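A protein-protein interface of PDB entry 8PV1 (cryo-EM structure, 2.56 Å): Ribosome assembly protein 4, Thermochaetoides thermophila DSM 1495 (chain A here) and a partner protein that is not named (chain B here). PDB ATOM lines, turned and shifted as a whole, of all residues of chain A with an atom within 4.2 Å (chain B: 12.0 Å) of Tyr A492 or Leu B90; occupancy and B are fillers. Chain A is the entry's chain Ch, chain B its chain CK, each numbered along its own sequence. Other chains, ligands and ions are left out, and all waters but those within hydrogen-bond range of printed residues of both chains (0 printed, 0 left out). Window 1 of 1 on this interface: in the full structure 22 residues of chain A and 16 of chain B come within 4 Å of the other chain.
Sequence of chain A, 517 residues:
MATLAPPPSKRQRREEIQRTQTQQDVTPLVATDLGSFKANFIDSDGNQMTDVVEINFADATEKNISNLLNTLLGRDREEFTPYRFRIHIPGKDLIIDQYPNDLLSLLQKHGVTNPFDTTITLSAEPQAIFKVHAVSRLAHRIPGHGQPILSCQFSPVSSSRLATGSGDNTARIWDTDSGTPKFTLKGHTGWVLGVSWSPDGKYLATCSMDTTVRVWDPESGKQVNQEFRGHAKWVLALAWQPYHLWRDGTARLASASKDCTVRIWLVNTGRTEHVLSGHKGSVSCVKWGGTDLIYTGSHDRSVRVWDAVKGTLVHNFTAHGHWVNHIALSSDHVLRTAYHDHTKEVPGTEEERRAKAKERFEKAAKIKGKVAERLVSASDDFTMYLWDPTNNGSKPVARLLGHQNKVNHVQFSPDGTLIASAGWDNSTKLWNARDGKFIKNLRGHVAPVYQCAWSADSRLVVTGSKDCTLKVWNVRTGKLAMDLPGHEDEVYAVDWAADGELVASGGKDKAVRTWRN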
ATOM      1  N   PRO A 148      -3.780  19.865  32.110  1.00  0.00           N
ATOM      2  CA  PRO A 148      -4.883  18.978  32.503  1.00  0.00           C
ATOM      3  C   PRO A 148      -4.515  17.996  33.608  1.00  0.00           C
ATOM      4  O   PRO A 148      -3.388  17.503  33.685  1.00  0.00           O
ATOM      5  CB  PRO A 148      -5.217  18.245  31.202  1.00  0.00           C
ATOM      6  CG  PRO A 148      -4.906  19.223  30.160  1.00  0.00           C
ATOM      7  CD  PRO A 148      -3.696  19.971  30.639  1.00  0.00           C
ATOM      8  N   ILE A 149      -5.492  17.730  34.474  1.00  0.00           N
ATOM      9  CA  ILE A 149      -5.305  16.808  35.585  1.00  0.00           C
ATOM     10  C   ILE A 149      -5.455  15.381  35.083  1.00  0.00           C
ATOM     11  O   ILE A 149      -6.489  15.010  34.513  1.00  0.00           O
ATOM     12  CB  ILE A 149      -6.314  17.107  36.701  1.00  0.00           C
ATOM     13  CG1 ILE A 149      -6.200  18.565  37.137  1.00  0.00           C
ATOM     14  CG2 ILE A 149      -6.098  16.177  37.880  1.00  0.00           C
ATOM     15  CD1 ILE A 149      -7.317  19.003  38.025  1.00  0.00           C
ATOM     16  N   TRP A 424     -16.723   3.155  25.534  1.00  0.00           N
ATOM     17  CA  TRP A 424     -16.658   4.211  24.535  1.00  0.00           C
ATOM     18  C   TRP A 424     -17.931   4.308  23.710  1.00  0.00           C
ATOM     19  O   TRP A 424     -18.024   5.176  22.836  1.00  0.00           O
ATOM     20  CB  TRP A 424     -15.456   4.001  23.610  1.00  0.00           C
ATOM     21  CG  TRP A 424     -14.119   4.266  24.242  1.00  0.00           C
ATOM     22  CD1 TRP A 424     -13.626   3.717  25.388  1.00  0.00           C
ATOM     23  CD2 TRP A 424     -13.098   5.139  23.749  1.00  0.00           C
ATOM     24  NE1 TRP A 424     -12.367   4.196  25.643  1.00  0.00           N
ATOM     25  CE2 TRP A 424     -12.020   5.072  24.650  1.00  0.00           C
ATOM     26  CE3 TRP A 424     -12.993   5.973  22.633  1.00  0.00           C
ATOM     27  CZ2 TRP A 424     -10.852   5.806  24.471  1.00  0.00           C
ATOM     28  CZ3 TRP A 424     -11.833   6.702  22.458  1.00  0.00           C
ATOM     29  CH2 TRP A 424     -10.779   6.614  23.371  1.00  0.00           C
ATOM     30  N   TYR A 450     -15.231   7.767  30.487  1.00  0.00           N
ATOM     31  CA  TYR A 450     -13.853   7.418  30.793  1.00  0.00           C
ATOM     32  C   TYR A 450     -13.691   6.710  32.128  1.00  0.00           C
ATOM     33  O   TYR A 450     -12.941   5.730  32.199  1.00  0.00           O
ATOM     34  CB  TYR A 450     -12.964   8.663  30.763  1.00  0.00           C
ATOM     35  CG  TYR A 450     -12.654   9.142  29.366  1.00  0.00           C
ATOM     36  CD1 TYR A 450     -12.542   8.241  28.316  1.00  0.00           C
ATOM     37  CD2 TYR A 450     -12.454  10.489  29.100  1.00  0.00           C
ATOM     38  CE1 TYR A 450     -12.254   8.670  27.038  1.00  0.00           C
ATOM     39  CE2 TYR A 450     -12.163  10.925  27.824  1.00  0.00           C
ATOM     40  CZ  TYR A 450     -12.064  10.012  26.799  1.00  0.00           C
ATOM     41  OH  TYR A 450     -11.776  10.441  25.526  1.00  0.00           O
ATOM     42  N   GLN A 451     -14.358   7.158  33.190  1.00  0.00           N
ATOM     43  CA  GLN A 451     -14.113   6.514  34.475  1.00  0.00           C
ATOM     44  C   GLN A 451     -15.413   6.314  35.236  1.00  0.00           C
ATOM     45  O   GLN A 451     -16.397   7.023  35.022  1.00  0.00           O
ATOM     46  CB  GLN A 451     -13.121   7.308  35.331  1.00  0.00           C
ATOM     47  CG  GLN A 451     -11.669   7.112  34.935  1.00  0.00           C
ATOM     48  CD  GLN A 451     -10.714   7.404  36.066  1.00  0.00           C
ATOM     49  OE1 GLN A 451     -11.131   7.689  37.186  1.00  0.00           O
ATOM     50  NE2 GLN A 451      -9.420   7.333  35.782  1.00  0.00           N
ATOM     51  N   GLU A 490     -13.040  17.945  28.973  1.00  0.00           N
ATOM     52  CA  GLU A 490     -13.173  16.513  29.226  1.00  0.00           C
ATOM     53  C   GLU A 490     -12.699  16.146  30.627  1.00  0.00           C
ATOM     54  O   GLU A 490     -11.705  16.680  31.123  1.00  0.00           O
ATOM     55  CB  GLU A 490     -12.378  15.723  28.185  1.00  0.00           C
ATOM     56  CG  GLU A 490     -12.675  16.116  26.750  1.00  0.00           C
ATOM     57  CD  GLU A 490     -11.857  15.329  25.746  1.00  0.00           C
ATOM     58  OE1 GLU A 490     -11.291  14.284  26.127  1.00  0.00           O
ATOM     59  OE2 GLU A 490     -11.780  15.755  24.575  1.00  0.00           O
ATOM     60  N   VAL A 491     -13.421  15.229  31.265  1.00  0.00           N
ATOM     61  CA  VAL A 491     -13.090  14.764  32.607  1.00  0.00           C
ATOM     62  C   VAL A 491     -12.262  13.491  32.495  1.00  0.00           C
ATOM     63  O   VAL A 491     -12.696  12.510  31.880  1.00  0.00           O
ATOM     64  CB  VAL A 491     -14.362  14.520  33.436  1.00  0.00           C
ATOM     65  CG1 VAL A 491     -14.001  13.980  34.806  1.00  0.00           C
ATOM     66  CG2 VAL A 491     -15.167  15.797  33.563  1.00  0.00           C
ATOM     67  N   TYR A 492     -11.074  13.500  33.096  1.00  0.00           N
ATOM     68  CA  TYR A 492     -10.147  12.382  32.988  1.00  0.00           C
ATOM     69  C   TYR A 492     -10.120  11.472  34.204  1.00  0.00           C
ATOM     70  O   TYR A 492      -9.974  10.260  34.041  1.00  0.00           O
ATOM     71  CB  TYR A 492      -8.723  12.892  32.734  1.00  0.00           C
ATOM     72  CG  TYR A 492      -8.510  13.474  31.358  1.00  0.00           C
ATOM     73  CD1 TYR A 492      -9.220  13.002  30.262  1.00  0.00           C
ATOM     74  CD2 TYR A 492      -7.583  14.487  31.151  1.00  0.00           C
ATOM     75  CE1 TYR A 492      -9.021  13.529  29.004  1.00  0.00           C
ATOM     76  CE2 TYR A 492      -7.377  15.018  29.899  1.00  0.00           C
ATOM     77  CZ  TYR A 492      -8.097  14.537  28.829  1.00  0.00           C
ATOM     78  OH  TYR A 492      -7.891  15.068  27.579  1.00  0.00           O
ATOM     79  N   ALA A 493     -10.251  12.010  35.413  1.00  0.00           N
ATOM     80  CA  ALA A 493     -10.119  11.223  36.629  1.00  0.00           C
ATOM     81  C   ALA A 493     -11.260  11.538  37.584  1.00  0.00           C
ATOM     82  O   ALA A 493     -11.579  12.705  37.823  1.00  0.00           O
ATOM     83  CB  ALA A 493      -8.776  11.484  37.312  1.00  0.00           C
ATOM     84  N   GLY A 506     -11.321  15.593  37.914  1.00  0.00           N
ATOM     85  CA  GLY A 506     -10.294  16.402  37.283  1.00  0.00           C
ATOM     86  C   GLY A 506     -10.182  16.036  35.825  1.00  0.00           C
ATOM     87  O   GLY A 506     -10.442  14.895  35.431  1.00  0.00           O
ATOM     88  N   GLY A 507      -9.790  17.008  35.014  1.00  0.00           N
ATOM     89  CA  GLY A 507      -9.644  16.738  33.602  1.00  0.00           C
ATOM     90  C   GLY A 507      -8.946  17.825  32.818  1.00  0.00           C
ATOM     91  O   GLY A 507      -7.994  18.441  33.300  1.00  0.00           O
ATOM     92  N   LYS A 508      -9.436  18.079  31.606  1.00  0.00           N
ATOM     93  CA  LYS A 508      -8.774  18.989  30.682  1.00  0.00           C
ATOM     94  C   LYS A 508      -8.962  20.456  31.051  1.00  0.00           C
ATOM     95  O   LYS A 508      -8.297  21.317  30.464  1.00  0.00           O
ATOM     96  CB  LYS A 508      -9.287  18.729  29.267  1.00  0.00           C
ATOM     97  CG  LYS A 508      -8.287  18.964  28.157  1.00  0.00           C
ATOM     98  CD  LYS A 508      -8.880  18.526  26.832  1.00  0.00           C
ATOM     99  CE  LYS A 508      -8.032  18.980  25.664  1.00  0.00           C
ATOM    100  NZ  LYS A 508      -8.697  18.681  24.369  1.00  0.00           N
ATOM    101  N   PRO B  82       3.744  12.647  23.067  1.00  0.00           N
ATOM    102  CA  PRO B  82       2.617  13.459  22.594  1.00  0.00           C
ATOM    103  C   PRO B  82       2.777  14.936  22.944  1.00  0.00           C
ATOM    104  O   PRO B  82       3.750  15.309  23.598  1.00  0.00           O
ATOM    105  CB  PRO B  82       1.418  12.850  23.326  1.00  0.00           C
ATOM    106  CG  PRO B  82       1.828  11.451  23.615  1.00  0.00           C
ATOM    107  CD  PRO B  82       3.298  11.517  23.898  1.00  0.00           C
ATOM    108  N   SER B  83       1.827  15.762  22.509  1.00  0.00           N
ATOM    109  CA  SER B  83       1.894  17.197  22.757  1.00  0.00           C
ATOM    110  C   SER B  83       1.008  17.594  23.929  1.00  0.00           C
ATOM    111  O   SER B  83       1.484  18.193  24.900  1.00  0.00           O
ATOM    112  CB  SER B  83       1.491  17.973  21.502  1.00  0.00           C
ATOM    113  OG  SER B  83       2.337  17.655  20.412  1.00  0.00           O
ATOM    114  N   ASP B  84      -0.279  17.270  23.848  1.00  0.00           N
ATOM    115  CA  ASP B  84      -1.201  17.606  24.922  1.00  0.00           C
ATOM    116  C   ASP B  84      -1.182  16.518  25.993  1.00  0.00           C
ATOM    117  O   ASP B  84      -1.112  15.330  25.666  1.00  0.00           O
ATOM    118  CB  ASP B  84      -2.618  17.775  24.382  1.00  0.00           C
ATOM    119  CG  ASP B  84      -2.945  19.217  24.053  1.00  0.00           C
ATOM    120  OD1 ASP B  84      -4.049  19.473  23.529  1.00  0.00           O
ATOM    121  OD2 ASP B  84      -2.098  20.095  24.316  1.00  0.00           O
ATOM    122  N   PRO B  85      -1.226  16.897  27.271  1.00  0.00           N
ATOM    123  CA  PRO B  85      -1.229  15.894  28.344  1.00  0.00           C
ATOM    124  C   PRO B  85      -2.495  15.050  28.331  1.00  0.00           C
ATOM    125  O   PRO B  85      -3.610  15.567  28.426  1.00  0.00           O
ATOM    126  CB  PRO B  85      -1.132  16.744  29.617  1.00  0.00           C
ATOM    127  CG  PRO B  85      -0.515  18.018  29.171  1.00  0.00           C
ATOM    128  CD  PRO B  85      -1.050  18.259  27.796  1.00  0.00           C
ATOM    129  N   ILE B  86      -2.309  13.739  28.218  1.00  0.00           N
ATOM    130  CA  ILE B  86      -3.413  12.784  28.202  1.00  0.00           C
ATOM    131  C   ILE B  86      -3.129  11.716  29.248  1.00  0.00           C
ATOM    132  O   ILE B  86      -1.966  11.480  29.611  1.00  0.00           O
ATOM    133  CB  ILE B  86      -3.606  12.158  26.800  1.00  0.00           C
ATOM    134  CG1 ILE B  86      -2.270  11.671  26.241  1.00  0.00           C
ATOM    135  CG2 ILE B  86      -4.267  13.149  25.858  1.00  0.00           C
ATOM    136  CD1 ILE B  86      -2.391  10.948  24.927  1.00  0.00           C
ATOM    137  N   PRO B  87      -4.167  11.064  29.771  1.00  0.00           N
ATOM    138  CA  PRO B  87      -3.939   9.991  30.744  1.00  0.00           C
ATOM    139  C   PRO B  87      -3.353   8.740  30.105  1.00  0.00           C
ATOM    140  O   PRO B  87      -3.208   8.622  28.884  1.00  0.00           O
ATOM    141  CB  PRO B  87      -5.334   9.715  31.315  1.00  0.00           C
ATOM    142  CG  PRO B  87      -6.150  10.882  30.953  1.00  0.00           C
ATOM    143  CD  PRO B  87      -5.592  11.429  29.691  1.00  0.00           C
ATOM    144  N   SER B  88      -3.008   7.791  30.980  1.00  0.00           N
ATOM    145  CA  SER B  88      -2.337   6.573  30.544  1.00  0.00           C
ATOM    146  C   SER B  88      -3.243   5.698  29.689  1.00  0.00           C
ATOM    147  O   SER B  88      -2.764   5.031  28.765  1.00  0.00           O
ATOM    148  CB  SER B  88      -1.833   5.795  31.758  1.00  0.00           C
ATOM    149  OG  SER B  88      -2.906   5.429  32.605  1.00  0.00           O
ATOM    150  N   TYR B  89      -4.548   5.687  29.969  1.00  0.00           N
ATOM    151  CA  TYR B  89      -5.456   4.913  29.134  1.00  0.00           C
ATOM    152  C   TYR B  89      -5.689   5.550  27.771  1.00  0.00           C
ATOM    153  O   TYR B  89      -6.127   4.854  26.851  1.00  0.00           O
ATOM    154  CB  TYR B  89      -6.789   4.689  29.858  1.00  0.00           C
ATOM    155  CG  TYR B  89      -7.502   5.933  30.347  1.00  0.00           C
ATOM    156  CD1 TYR B  89      -8.321   6.672  29.502  1.00  0.00           C
ATOM    157  CD2 TYR B  89      -7.383   6.348  31.667  1.00  0.00           C
ATOM    158  CE1 TYR B  89      -8.979   7.797  29.949  1.00  0.00           C
ATOM    159  CE2 TYR B  89      -8.042   7.472  32.125  1.00  0.00           C
ATOM    160  CZ  TYR B  89      -8.838   8.193  31.261  1.00  0.00           C
ATOM    161  OH  TYR B  89      -9.496   9.312  31.708  1.00  0.00           O
ATOM    162  N   LEU B  90      -5.412   6.842  27.617  1.00  0.00           N
ATOM    163  CA  LEU B  90      -5.465   7.499  26.319  1.00  0.00           C
ATOM    164  C   LEU B  90      -4.114   7.525  25.618  1.00  0.00           C
ATOM    165  O   LEU B  90      -4.054   7.893  24.442  1.00  0.00           O
ATOM    166  CB  LEU B  90      -5.994   8.928  26.467  1.00  0.00           C
ATOM    167  CG  LEU B  90      -7.465   9.081  26.850  1.00  0.00           C
ATOM    168  CD1 LEU B  90      -7.876  10.540  26.815  1.00  0.00           C
ATOM    169  CD2 LEU B  90      -8.352   8.252  25.939  1.00  0.00           C
ATOM    170  N   LEU B  91      -3.041   7.149  26.308  1.00  0.00           N
ATOM    171  CA  LEU B  91      -1.733   7.052  25.671  1.00  0.00           C
ATOM    172  C   LEU B  91      -1.712   5.950  24.616  1.00  0.00           C
ATOM    173  O   LEU B  91      -2.459   4.971  24.692  1.00  0.00           O
ATOM    174  CB  LEU B  91      -0.646   6.787  26.711  1.00  0.00           C
ATOM    175  CG  LEU B  91      -0.186   7.988  27.538  1.00  0.00           C
ATOM    176  CD1 LEU B  91       0.814   7.556  28.593  1.00  0.00           C
ATOM    177  CD2 LEU B  91       0.408   9.055  26.640  1.00  0.00           C
ATOM    178  N   ASP B  92      -0.857   6.143  23.608  1.00  0.00           N
ATOM    179  CA  ASP B  92      -0.591   5.266  22.466  1.00  0.00           C
ATOM    180  C   ASP B  92      -1.779   5.093  21.526  1.00  0.00           C
ATOM    181  O   ASP B  92      -1.694   4.279  20.600  1.00  0.00           O
ATOM    182  CB  ASP B  92      -0.098   3.871  22.881  1.00  0.00           C
ATOM    183  CG  ASP B  92       1.290   3.898  23.480  1.00  0.00           C
ATOM    184  OD1 ASP B  92       2.081   4.789  23.107  1.00  0.00           O
ATOM    185  OD2 ASP B  92       1.594   3.025  24.318  1.00  0.00           O
ATOM    186  N   ARG B  93      -2.871   5.819  21.718  1.00  0.00           N
ATOM    187  CA  ARG B  93      -3.995   5.783  20.797  1.00  0.00           C
ATOM    188  C   ARG B  93      -3.857   6.889  19.760  1.00  0.00           C
ATOM    189  O   ARG B  93      -3.017   7.783  19.876  1.00  0.00           O
ATOM    190  CB  ARG B  93      -5.324   5.931  21.541  1.00  0.00           C
ATOM    191  CG  ARG B  93      -5.503   4.977  22.697  1.00  0.00           C
ATOM    192  CD  ARG B  93      -6.877   5.141  23.320  1.00  0.00           C
ATOM    193  NE  ARG B  93      -7.131   4.150  24.356  1.00  0.00           N
ATOM    194  CZ  ARG B  93      -7.580   2.924  24.124  1.00  0.00           C
ATOM    195  NH1 ARG B  93      -7.838   2.503  22.899  1.00  0.00           N
ATOM    196  NH2 ARG B  93      -7.776   2.101  25.150  1.00  0.00           N
ATOM    197  N   ALA B  94      -4.700   6.817  18.735  1.00  0.00           N
ATOM    198  CA  ALA B  94      -4.723   7.844  17.700  1.00  0.00           C
ATOM    199  C   ALA B  94      -5.568   9.016  18.179  1.00  0.00           C
ATOM    200  O   ALA B  94      -6.799   8.984  18.084  1.00  0.00           O
ATOM    201  CB  ALA B  94      -5.268   7.271  16.396  1.00  0.00           C
ATOM    202  N   ASN B  95      -4.912  10.051  18.697  1.00  0.00           N
ATOM    203  CA  ASN B  95      -5.593  11.216  19.225  1.00  0.00           C
ATOM    204  C   ASN B  95      -5.532  12.350  18.211  1.00  0.00           C
ATOM    205  O   ASN B  95      -4.558  12.439  17.449  1.00  0.00           O
ATOM    206  CB  ASN B  95      -4.960  11.669  20.553  1.00  0.00           C
ATOM    207  CG  ASN B  95      -5.001  10.590  21.619  1.00  0.00           C
ATOM    208  OD1 ASN B  95      -4.074   9.791  21.746  1.00  0.00           O
ATOM    209  ND2 ASN B  95      -6.079  10.563  22.392  1.00  0.00           N
ATOM    210  N   PRO B  96      -6.548  13.210  18.145  1.00  0.00           N
ATOM    211  CA  PRO B  96      -6.481  14.370  17.250  1.00  0.00           C
ATOM    212  C   PRO B  96      -5.394  15.345  17.682  1.00  0.00           C
ATOM    213  O   PRO B  96      -5.049  15.439  18.862  1.00  0.00           O
ATOM    214  CB  PRO B  96      -7.876  14.992  17.373  1.00  0.00           C
ATOM    215  CG  PRO B  96      -8.752  13.878  17.832  1.00  0.00           C
ATOM    216  CD  PRO B  96      -7.891  13.034  18.722  1.00  0.00           C
ATOM    217  N   THR B  97      -4.843  16.066  16.702  1.00  0.00           N
ATOM    218  CA  THR B  97      -3.776  17.021  16.984  1.00  0.00           C
ATOM    219  C   THR B  97      -4.284  18.205  17.796  1.00  0.00           C
ATOM    220  O   THR B  97      -3.559  18.734  18.649  1.00  0.00           O
ATOM    221  CB  THR B  97      -3.146  17.505  15.677  1.00  0.00           C
ATOM    222  OG1 THR B  97      -4.131  18.190  14.896  1.00  0.00           O
ATOM    223  CG2 THR B  97      -2.603  16.327  14.880  1.00  0.00           C
ATOM    224  N   THR B  98      -5.531  18.624  17.541  1.00  0.00           N
ATOM    225  CA  THR B  98      -6.183  19.763  18.205  1.00  0.00           C
ATOM    226  C   THR B  98      -5.347  21.038  18.048  1.00  0.00           C
ATOM    227  O   THR B  98      -4.760  21.544  19.008  1.00  0.00           O
ATOM    228  CB  THR B  98      -6.487  19.458  19.678  1.00  0.00           C
ATOM    229  OG1 THR B  98      -7.132  18.183  19.766  1.00  0.00           O
ATOM    230  CG2 THR B  98      -7.455  20.489  20.260  1.00  0.00           C
ATOM    231  N   THR B 188     -12.673  23.468  17.240  1.00  0.00           N
ATOM    232  CA  THR B 188     -11.981  23.279  18.511  1.00  0.00           C
ATOM    233  C   THR B 188     -11.538  21.831  18.691  1.00  0.00           C
ATOM    234  O   THR B 188     -10.380  21.564  19.028  1.00  0.00           O
ATOM    235  CB  THR B 188     -12.880  23.714  19.667  1.00  0.00           C
ATOM    236  OG1 THR B 188     -13.494  24.970  19.351  1.00  0.00           O
ATOM    237  CG2 THR B 188     -12.071  23.858  20.945  1.00  0.00           C
ATOM    238  N   LEU B 189     -12.449  20.879  18.472  1.00  0.00           N
ATOM    239  CA  LEU B 189     -12.128  19.477  18.708  1.00  0.00           C
ATOM    240  C   LEU B 189     -11.329  18.854  17.573  1.00  0.00           C
ATOM    241  O   LEU B 189     -10.806  17.748  17.748  1.00  0.00           O
ATOM    242  CB  LEU B 189     -13.408  18.675  18.934  1.00  0.00           C
ATOM    243  CG  LEU B 189     -14.408  19.271  19.923  1.00  0.00           C
ATOM    244  CD1 LEU B 189     -15.669  18.428  19.974  1.00  0.00           C
ATOM    245  CD2 LEU B 189     -13.785  19.396  21.302  1.00  0.00           C
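The side-chain hydroxyl (OH) of Tyr B89 lies within hydrogen-bond range of the backbone carbonyl oxygen (O) of Tyr A492.
O of Tyr B89 sits at hydrogen-bond distance from NE of Arg B93 (2.8 Å).
The backbone carbonyl oxygen (O) of Leu B90 lies close to the side-chain amide oxygen (OD1) of Asn B95 (3.3 Å).
NE2 of Gln A451 is in hydrogen-bond range of O of Tyr A492 (3.5 Å).
The backbone NH (N) of Tyr A492 sits at hydrogen-bond distance from the backbone carbonyl oxygen (O) of Gly A506.
Among the printed residues, pairs that only touch across the chains: Tyr A492 with Pro B87, Tyr A450 with Tyr B89, Trp A424 with Leu B90, Tyr A492 with Leu B90 and Gln A451 with Tyr B89.
Pro A148 touches none of the printed residues of chain B.
Of the printed residues of chain B, Trp A424 touches Leu B90.
Of chain B, only Tyr B89 (3.9 Å) comes within 4 Å of Gln A451.
No residue of chain B comes within 4 Å of Glu A490.
Of chain B, only Pro B87, Tyr B89 and Leu B90 come within 4 Å of Tyr A492.
No residue of chain B comes within 4 Å of Ala A493.
No residue of chain B comes within 4 Å of Gly A506.
No residue of chain B comes within 4 Å of Gly A507.
No residue of chain B comes within 4 Å of Lys A508.
Of the printed residues of chain A, Pro B87 touches Tyr A492.
Ser B88 touches none of the printed residues of chain A.
Of the printed residues of chain A, Tyr B89 touches Tyr A450, Gln A451 and Tyr A492.
Leu B90 touches two residues of chain A.
The nearest residue of chain B that does not touch Tyr A492 is Pro B85 (4.1 Å).
The nearest residue of chain A that does not touch Leu B90 is Tyr A450 (4.1 Å).
Of the 19 printed residues of chain B, 3 touch a printed residue of chain A.
Hydrophobic or aromatic side chains of chain B within 4 Å of the printed part of chain A: Pro B87, Tyr B89 and Leu B90.
Along chain B the printed residues that touch a printed residue of chain A span positions 87 to 90.
Of the 12 printed residues of chain A, 4 touch a printed residue of chain B.
Hydrophobic or aromatic side chains of chain A that line the printed part of chain B: Trp A424, Tyr A450 and Tyr A492.
Along chain A the printed residues that touch a printed residue of chain B span positions 424 to 492.
Among the printed residues, 6 pairs touch across the chains.
Among the printed residues, no Asp or Glu carboxylate lies within 4 Å of a Lys or Arg side-chain nitrogen of the other chain.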
